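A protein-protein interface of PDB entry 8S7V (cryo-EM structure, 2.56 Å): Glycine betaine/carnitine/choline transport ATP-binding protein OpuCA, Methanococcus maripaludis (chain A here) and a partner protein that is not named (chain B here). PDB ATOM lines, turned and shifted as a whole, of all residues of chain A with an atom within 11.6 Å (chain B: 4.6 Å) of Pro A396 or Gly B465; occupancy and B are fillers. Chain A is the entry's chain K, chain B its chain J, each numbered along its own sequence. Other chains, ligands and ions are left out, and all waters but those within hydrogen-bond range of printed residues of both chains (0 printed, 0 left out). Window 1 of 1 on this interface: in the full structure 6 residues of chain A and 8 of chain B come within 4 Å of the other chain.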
ATOM      1  N   LEU A 384     -25.470  17.071  -8.491  1.00  0.00           N
ATOM      2  CA  LEU A 384     -24.721  15.820  -8.546  1.00  0.00           C
ATOM      3  C   LEU A 384     -25.657  14.623  -8.649  1.00  0.00           C
ATOM      4  O   LEU A 384     -25.424  13.707  -9.448  1.00  0.00           O
ATOM      5  CB  LEU A 384     -23.830  15.696  -7.311  1.00  0.00           C
ATOM      6  CG  LEU A 384     -22.960  14.447  -7.184  1.00  0.00           C
ATOM      7  CD1 LEU A 384     -22.123  14.250  -8.431  1.00  0.00           C
ATOM      8  CD2 LEU A 384     -22.080  14.538  -5.951  1.00  0.00           C
ATOM      9  N   LEU A 387     -27.078  14.400 -12.157  1.00  0.00           N
ATOM     10  CA  LEU A 387     -26.159  13.845 -13.146  1.00  0.00           C
ATOM     11  C   LEU A 387     -25.943  12.349 -12.948  1.00  0.00           C
ATOM     12  O   LEU A 387     -25.849  11.600 -13.927  1.00  0.00           O
ATOM     13  CB  LEU A 387     -24.818  14.576 -13.113  1.00  0.00           C
ATOM     14  CG  LEU A 387     -24.647  15.837 -13.966  1.00  0.00           C
ATOM     15  CD1 LEU A 387     -25.626  15.844 -15.130  1.00  0.00           C
ATOM     16  CD2 LEU A 387     -24.773  17.098 -13.145  1.00  0.00           C
ATOM     17  N   THR A 388     -25.858  11.889 -11.700  1.00  0.00           N
ATOM     18  CA  THR A 388     -25.371  10.543 -11.424  1.00  0.00           C
ATOM     19  C   THR A 388     -26.475   9.558 -11.061  1.00  0.00           C
ATOM     20  O   THR A 388     -26.622   8.529 -11.726  1.00  0.00           O
ATOM     21  CB  THR A 388     -24.321  10.597 -10.309  1.00  0.00           C
ATOM     22  OG1 THR A 388     -24.952  10.942  -9.070  1.00  0.00           O
ATOM     23  CG2 THR A 388     -23.262  11.631 -10.638  1.00  0.00           C
ATOM     24  N   GLU A 389     -27.263   9.837 -10.025  1.00  0.00           N
ATOM     25  CA  GLU A 389     -28.185   8.837  -9.502  1.00  0.00           C
ATOM     26  C   GLU A 389     -29.565   8.879 -10.141  1.00  0.00           C
ATOM     27  O   GLU A 389     -30.254   7.854 -10.155  1.00  0.00           O
ATOM     28  CB  GLU A 389     -28.331   8.998  -7.986  1.00  0.00           C
ATOM     29  CG  GLU A 389     -27.018   9.226  -7.260  1.00  0.00           C
ATOM     30  CD  GLU A 389     -27.125   8.982  -5.770  1.00  0.00           C
ATOM     31  OE1 GLU A 389     -27.889   8.082  -5.367  1.00  0.00           O
ATOM     32  OE2 GLU A 389     -26.446   9.693  -4.999  1.00  0.00           O
ATOM     33  N   GLY A 392     -28.876   6.932 -13.491  1.00  0.00           N
ATOM     34  CA  GLY A 392     -28.200   5.629 -13.331  1.00  0.00           C
ATOM     35  C   GLY A 392     -26.885   5.573 -14.086  1.00  0.00           C
ATOM     36  O   GLY A 392     -26.878   5.041 -15.211  1.00  0.00           O
ATOM     37  N   LEU A 393     -25.809   6.092 -13.487  1.00  0.00           N
ATOM     38  CA  LEU A 393     -24.469   6.060 -14.131  1.00  0.00           C
ATOM     39  C   LEU A 393     -23.838   4.681 -13.909  1.00  0.00           C
ATOM     40  O   LEU A 393     -24.009   4.124 -12.810  1.00  0.00           O
ATOM     41  CB  LEU A 393     -23.601   7.161 -13.516  1.00  0.00           C
ATOM     42  CG  LEU A 393     -23.041   8.181 -14.503  1.00  0.00           C
ATOM     43  CD1 LEU A 393     -24.164   8.833 -15.295  1.00  0.00           C
ATOM     44  CD2 LEU A 393     -22.217   9.232 -13.777  1.00  0.00           C
ATOM     45  N   GLU A 394     -23.127   4.163 -14.913  1.00  0.00           N
ATOM     46  CA  GLU A 394     -22.505   2.814 -14.802  1.00  0.00           C
ATOM     47  C   GLU A 394     -21.121   2.940 -14.161  1.00  0.00           C
ATOM     48  O   GLU A 394     -20.126   2.789 -14.893  1.00  0.00           O
ATOM     49  CB  GLU A 394     -22.474   2.134 -16.170  1.00  0.00           C
ATOM     50  CG  GLU A 394     -23.393   0.929 -16.248  1.00  0.00           C
ATOM     51  CD  GLU A 394     -24.463   1.016 -17.320  1.00  0.00           C
ATOM     52  OE1 GLU A 394     -25.122   2.068 -17.408  1.00  0.00           O
ATOM     53  OE2 GLU A 394     -24.628   0.033 -18.066  1.00  0.00           O
ATOM     54  N   MET A 395     -21.068   3.190 -12.850  1.00  0.00           N
ATOM     55  CA  MET A 395     -19.830   3.308 -12.090  1.00  0.00           C
ATOM     56  C   MET A 395     -20.188   3.406 -10.610  1.00  0.00           C
ATOM     57  O   MET A 395     -21.309   3.790 -10.269  1.00  0.00           O
ATOM     58  CB  MET A 395     -19.009   4.531 -12.531  1.00  0.00           C
ATOM     59  CG  MET A 395     -19.602   5.867 -12.131  1.00  0.00           C
ATOM     60  SD  MET A 395     -18.897   7.233 -13.072  1.00  0.00           S
ATOM     61  CE  MET A 395     -18.492   6.418 -14.612  1.00  0.00           C
ATOM     62  N   PRO A 396     -19.256   3.056  -9.723  1.00  0.00           N
ATOM     63  CA  PRO A 396     -19.517   3.211  -8.289  1.00  0.00           C
ATOM     64  C   PRO A 396     -19.713   4.673  -7.920  1.00  0.00           C
ATOM     65  O   PRO A 396     -19.232   5.580  -8.601  1.00  0.00           O
ATOM     66  CB  PRO A 396     -18.259   2.631  -7.634  1.00  0.00           C
ATOM     67  CG  PRO A 396     -17.694   1.711  -8.655  1.00  0.00           C
ATOM     68  CD  PRO A 396     -17.993   2.343  -9.977  1.00  0.00           C
ATOM     69  N   GLY A 397     -20.436   4.893  -6.820  1.00  0.00           N
ATOM     70  CA  GLY A 397     -20.803   6.239  -6.417  1.00  0.00           C
ATOM     71  C   GLY A 397     -19.633   7.148  -6.109  1.00  0.00           C
ATOM     72  O   GLY A 397     -19.781   8.373  -6.188  1.00  0.00           O
ATOM     73  N   GLU A 398     -18.477   6.584  -5.757  1.00  0.00           N
ATOM     74  CA  GLU A 398     -17.329   7.425  -5.436  1.00  0.00           C
ATOM     75  C   GLU A 398     -16.734   8.079  -6.676  1.00  0.00           C
ATOM     76  O   GLU A 398     -16.295   9.233  -6.612  1.00  0.00           O
ATOM     77  CB  GLU A 398     -16.262   6.611  -4.708  1.00  0.00           C
ATOM     78  CG  GLU A 398     -15.297   7.465  -3.908  1.00  0.00           C
ATOM     79  CD  GLU A 398     -14.092   6.689  -3.429  1.00  0.00           C
ATOM     80  OE1 GLU A 398     -14.259   5.506  -3.066  1.00  0.00           O
ATOM     81  OE2 GLU A 398     -12.981   7.257  -3.416  1.00  0.00           O
ATOM     82  N   PHE A 399     -16.706   7.369  -7.801  1.00  0.00           N
ATOM     83  CA  PHE A 399     -16.131   7.892  -9.031  1.00  0.00           C
ATOM     84  C   PHE A 399     -17.145   8.618  -9.902  1.00  0.00           C
ATOM     85  O   PHE A 399     -16.788   9.080 -10.989  1.00  0.00           O
ATOM     86  CB  PHE A 399     -15.477   6.761  -9.833  1.00  0.00           C
ATOM     87  CG  PHE A 399     -14.658   5.824  -8.997  1.00  0.00           C
ATOM     88  CD1 PHE A 399     -13.532   6.275  -8.332  1.00  0.00           C
ATOM     89  CD2 PHE A 399     -15.010   4.491  -8.880  1.00  0.00           C
ATOM     90  CE1 PHE A 399     -12.774   5.417  -7.562  1.00  0.00           C
ATOM     91  CE2 PHE A 399     -14.255   3.628  -8.112  1.00  0.00           C
ATOM     92  CZ  PHE A 399     -13.135   4.092  -7.451  1.00  0.00           C
ATOM     93  N   ALA A 400     -18.397   8.725  -9.457  1.00  0.00           N
ATOM     94  CA  ALA A 400     -19.400   9.462 -10.213  1.00  0.00           C
ATOM     95  C   ALA A 400     -19.243  10.970 -10.081  1.00  0.00           C
ATOM     96  O   ALA A 400     -19.589  11.697 -11.018  1.00  0.00           O
ATOM     97  CB  ALA A 400     -20.802   9.048  -9.769  1.00  0.00           C
ATOM     98  N   LYS A 401     -18.735  11.454  -8.945  1.00  0.00           N
ATOM     99  CA  LYS A 401     -18.584  12.893  -8.752  1.00  0.00           C
ATOM    100  C   LYS A 401     -17.584  13.482  -9.740  1.00  0.00           C
ATOM    101  O   LYS A 401     -17.817  14.552 -10.314  1.00  0.00           O
ATOM    102  CB  LYS A 401     -18.158  13.183  -7.314  1.00  0.00           C
ATOM    103  CG  LYS A 401     -18.070  14.662  -6.986  1.00  0.00           C
ATOM    104  CD  LYS A 401     -18.349  14.921  -5.517  1.00  0.00           C
ATOM    105  CE  LYS A 401     -17.922  16.324  -5.119  1.00  0.00           C
ATOM    106  NZ  LYS A 401     -16.452  16.419  -4.913  1.00  0.00           N
ATOM    107  N   MET A 402     -16.458  12.795  -9.949  1.00  0.00           N
ATOM    108  CA  MET A 402     -15.465  13.291 -10.897  1.00  0.00           C
ATOM    109  C   MET A 402     -15.985  13.248 -12.328  1.00  0.00           C
ATOM    110  O   MET A 402     -15.707  14.163 -13.112  1.00  0.00           O
ATOM    111  CB  MET A 402     -14.169  12.493 -10.771  1.00  0.00           C
ATOM    112  CG  MET A 402     -13.862  12.029  -9.355  1.00  0.00           C
ATOM    113  SD  MET A 402     -12.999  10.448  -9.303  1.00  0.00           S
ATOM    114  CE  MET A 402     -11.335  10.959  -9.725  1.00  0.00           C
ATOM    115  N   LYS A 403     -16.741  12.207 -12.685  1.00  0.00           N
ATOM    116  CA  LYS A 403     -17.344  12.151 -14.013  1.00  0.00           C
ATOM    117  C   LYS A 403     -18.332  13.294 -14.210  1.00  0.00           C
ATOM    118  O   LYS A 403     -18.374  13.922 -15.275  1.00  0.00           O
ATOM    119  CB  LYS A 403     -18.030  10.800 -14.215  1.00  0.00           C
ATOM    120  CG  LYS A 403     -18.882  10.715 -15.467  1.00  0.00           C
ATOM    121  CD  LYS A 403     -18.098  10.111 -16.618  1.00  0.00           C
ATOM    122  CE  LYS A 403     -18.831  10.278 -17.938  1.00  0.00           C
ATOM    123  NZ  LYS A 403     -18.536  11.591 -18.573  1.00  0.00           N
ATOM    124  N   ALA A 404     -19.140  13.580 -13.185  1.00  0.00           N
ATOM    125  CA  ALA A 404     -20.083  14.691 -13.270  1.00  0.00           C
ATOM    126  C   ALA A 404     -19.358  16.022 -13.415  1.00  0.00           C
ATOM    127  O   ALA A 404     -19.774  16.877 -14.206  1.00  0.00           O
ATOM    128  CB  ALA A 404     -20.992  14.705 -12.041  1.00  0.00           C
ATOM    129  N   GLU A 405     -18.278  16.219 -12.657  1.00  0.00           N
ATOM    130  CA  GLU A 405     -17.504  17.451 -12.778  1.00  0.00           C
ATOM    131  C   GLU A 405     -16.899  17.585 -14.169  1.00  0.00           C
ATOM    132  O   GLU A 405     -16.902  18.675 -14.755  1.00  0.00           O
ATOM    133  CB  GLU A 405     -16.411  17.492 -11.714  1.00  0.00           C
ATOM    134  CG  GLU A 405     -16.692  18.453 -10.576  1.00  0.00           C
ATOM    135  CD  GLU A 405     -15.722  18.290  -9.424  1.00  0.00           C
ATOM    136  OE1 GLU A 405     -15.439  17.135  -9.043  1.00  0.00           O
ATOM    137  OE2 GLU A 405     -15.242  19.317  -8.899  1.00  0.00           O
ATOM    138  N   ILE A 444     -23.889  12.974 -20.510  1.00  0.00           N
ATOM    139  CA  ILE A 444     -23.086  12.128 -19.633  1.00  0.00           C
ATOM    140  C   ILE A 444     -23.270  10.644 -19.926  1.00  0.00           C
ATOM    141  O   ILE A 444     -22.350   9.854 -19.686  1.00  0.00           O
ATOM    142  CB  ILE A 444     -23.398  12.450 -18.159  1.00  0.00           C
ATOM    143  CG1 ILE A 444     -22.311  11.891 -17.241  1.00  0.00           C
ATOM    144  CG2 ILE A 444     -24.760  11.923 -17.764  1.00  0.00           C
ATOM    145  CD1 ILE A 444     -22.421  12.366 -15.812  1.00  0.00           C
ATOM    146  N   ILE B 410      -7.757   2.272  -3.559  1.00  0.00           N
ATOM    147  CA  ILE B 410      -8.791   1.254  -3.678  1.00  0.00           C
ATOM    148  C   ILE B 410      -8.309   0.114  -4.569  1.00  0.00           C
ATOM    149  O   ILE B 410      -7.659   0.317  -5.598  1.00  0.00           O
ATOM    150  CB  ILE B 410     -10.095   1.871  -4.216  1.00  0.00           C
ATOM    151  CG1 ILE B 410     -10.729   2.773  -3.162  1.00  0.00           C
ATOM    152  CG2 ILE B 410     -11.080   0.798  -4.647  1.00  0.00           C
ATOM    153  CD1 ILE B 410     -12.075   3.302  -3.570  1.00  0.00           C
ATOM    154  N   TYR B 447     -23.690  -2.778  -8.350  1.00  0.00           N
ATOM    155  CA  TYR B 447     -22.572  -3.718  -8.431  1.00  0.00           C
ATOM    156  C   TYR B 447     -22.536  -4.581  -7.170  1.00  0.00           C
ATOM    157  O   TYR B 447     -21.643  -4.494  -6.327  1.00  0.00           O
ATOM    158  CB  TYR B 447     -21.267  -2.967  -8.651  1.00  0.00           C
ATOM    159  CG  TYR B 447     -21.285  -2.164  -9.924  1.00  0.00           C
ATOM    160  CD1 TYR B 447     -21.227  -2.793 -11.157  1.00  0.00           C
ATOM    161  CD2 TYR B 447     -21.384  -0.781  -9.897  1.00  0.00           C
ATOM    162  CE1 TYR B 447     -21.255  -2.073 -12.326  1.00  0.00           C
ATOM    163  CE2 TYR B 447     -21.413  -0.050 -11.065  1.00  0.00           C
ATOM    164  CZ  TYR B 447     -21.348  -0.703 -12.276  1.00  0.00           C
ATOM    165  OH  TYR B 447     -21.376   0.010 -13.447  1.00  0.00           O
ATOM    166  N   TYR B 461     -17.376   6.678   2.088  1.00  0.00           N
ATOM    167  CA  TYR B 461     -17.459   5.580   1.138  1.00  0.00           C
ATOM    168  C   TYR B 461     -16.761   4.342   1.683  1.00  0.00           C
ATOM    169  O   TYR B 461     -15.749   4.433   2.381  1.00  0.00           O
ATOM    170  CB  TYR B 461     -16.837   5.977  -0.202  1.00  0.00           C
ATOM    171  CG  TYR B 461     -17.664   6.971  -0.981  1.00  0.00           C
ATOM    172  CD1 TYR B 461     -18.871   6.602  -1.553  1.00  0.00           C
ATOM    173  CD2 TYR B 461     -17.242   8.284  -1.128  1.00  0.00           C
ATOM    174  CE1 TYR B 461     -19.630   7.509  -2.262  1.00  0.00           C
ATOM    175  CE2 TYR B 461     -17.994   9.199  -1.835  1.00  0.00           C
ATOM    176  CZ  TYR B 461     -19.187   8.806  -2.398  1.00  0.00           C
ATOM    177  OH  TYR B 461     -19.942   9.715  -3.104  1.00  0.00           O
ATOM    178  N   GLY B 462     -17.314   3.180   1.351  1.00  0.00           N
ATOM    179  CA  GLY B 462     -16.740   1.920   1.753  1.00  0.00           C
ATOM    180  C   GLY B 462     -15.575   1.527   0.870  1.00  0.00           C
ATOM    181  O   GLY B 462     -15.172   2.269  -0.030  1.00  0.00           O
ATOM    182  N   PRO B 463     -15.010   0.339   1.110  1.00  0.00           N
ATOM    183  CA  PRO B 463     -13.852  -0.106   0.321  1.00  0.00           C
ATOM    184  C   PRO B 463     -14.158  -0.378  -1.142  1.00  0.00           C
ATOM    185  O   PRO B 463     -13.239  -0.732  -1.888  1.00  0.00           O
ATOM    186  CB  PRO B 463     -13.423  -1.399   1.034  1.00  0.00           C
ATOM    187  CG  PRO B 463     -14.051  -1.329   2.386  1.00  0.00           C
ATOM    188  CD  PRO B 463     -15.337  -0.603   2.188  1.00  0.00           C
ATOM    189  N   THR B 464     -15.407  -0.229  -1.583  1.00  0.00           N
ATOM    190  CA  THR B 464     -15.782  -0.531  -2.957  1.00  0.00           C
ATOM    191  C   THR B 464     -16.405   0.658  -3.676  1.00  0.00           C
ATOM    192  O   THR B 464     -16.990   0.478  -4.750  1.00  0.00           O
ATOM    193  CB  THR B 464     -16.750  -1.717  -2.996  1.00  0.00           C
ATOM    194  OG1 THR B 464     -17.797  -1.503  -2.041  1.00  0.00           O
ATOM    195  CG2 THR B 464     -16.024  -3.005  -2.661  1.00  0.00           C
ATOM    196  N   GLY B 465     -16.301   1.862  -3.119  1.00  0.00           N
ATOM    197  CA  GLY B 465     -16.841   3.039  -3.763  1.00  0.00           C
ATOM    198  C   GLY B 465     -18.314   3.285  -3.537  1.00  0.00           C
ATOM    199  O   GLY B 465     -18.862   4.227  -4.117  1.00  0.00           O
ATOM    200  N   GLU B 466     -18.974   2.474  -2.719  1.00  0.00           N
ATOM    201  CA  GLU B 466     -20.384   2.646  -2.405  1.00  0.00           C
ATOM    202  C   GLU B 466     -20.538   3.219  -1.004  1.00  0.00           C
ATOM    203  O   GLU B 466     -19.625   3.166  -0.176  1.00  0.00           O
ATOM    204  CB  GLU B 466     -21.140   1.318  -2.523  1.00  0.00           C
ATOM    205  CG  GLU B 466     -20.785   0.494  -3.748  1.00  0.00           C
ATOM    206  CD  GLU B 466     -21.460   1.000  -5.006  1.00  0.00           C
ATOM    207  OE1 GLU B 466     -22.364   1.853  -4.896  1.00  0.00           O
ATOM    208  OE2 GLU B 466     -21.090   0.540  -6.105  1.00  0.00           O
ATOM    209  N   THR B 467     -21.720   3.771  -0.744  1.00  0.00           N
ATOM    210  CA  THR B 467     -22.021   4.320   0.568  1.00  0.00           C
ATOM    211  C   THR B 467     -22.169   3.189   1.586  1.00  0.00           C
ATOM    212  O   THR B 467     -22.195   2.004   1.246  1.00  0.00           O
ATOM    213  CB  THR B 467     -23.279   5.179   0.508  1.00  0.00           C
ATOM    214  OG1 THR B 467     -24.242   4.558  -0.351  1.00  0.00           O
ATOM    215  CG2 THR B 467     -22.949   6.562  -0.027  1.00  0.00           C
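Hydrophobic or aromatic side chains of chain A that line the printed part of chain B: Pro A396. Among the printed residues, no Asp or Glu carboxylate lies within 4 Å of a Lys or Arg side-chain nitrogen of the other chain.
Among the printed residues, merely in contact across the chains: Glu A398 with Ile B410 (3.1 Å), Glu A398 with Tyr B461 (3.5 Å), Pro A396 with Glu B466 (3.8 Å), Pro A396 with Thr B464 (3.8 Å) and Pro A396 with Gly B465 (3.9 Å).
Of the printed residues of chain B, Pro A396 touches Thr B464, Gly B465 and Glu B466. Gly B465 touches just these residues of chain A: Pro A396, Gly A397 and Glu A398. Tyr B461 touches just these residues of chain A: Gly A397 (3.4 Å) and Glu A398 (3.5 Å). Gly B462 touches none of the printed residues of chain A. Of the printed residues of chain A, Thr B464 touches Pro A396 (3.8 Å). Glu B466 touches one residue of chain A. Of the printed residues of chain A, Tyr B447 touches Glu A394 (3.0 Å) and Met A395 (3.3 Å). Of the printed residues of chain A, Ile B410 touches Glu A398 (3.1 Å). Of the printed residues of chain B, Glu A394 touches Tyr B447 (3.0 Å). Printed residues of chain B within 4 Å of Glu A398: Ile B410 (3.1 Å), Tyr B461 (3.5 Å) and Gly B465 (2.9 Å). Glu A405 touches none of the printed residues of chain B. The nearest residue of chain A that does not touch Gly B465 is Phe A399 (5.1 Å).
The backbone carbonyl oxygen of Glu A394 lies close to the side-chain hydroxyl of Tyr B447. N of Met A395 sits at hydrogen-bond distance from OH of Tyr B447 (3.3 Å). O of Gly A397 lies within hydrogen-bond range of OH of Tyr B461, 3.4 Å away. The backbone NH (N) of Gly A397 is in hydrogen-bond range of the backbone carbonyl oxygen (O) of Gly B465, 3.2 Å away. The backbone NH of Glu A398 is in hydrogen-bond range of the backbone carbonyl oxygen of Gly B465.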
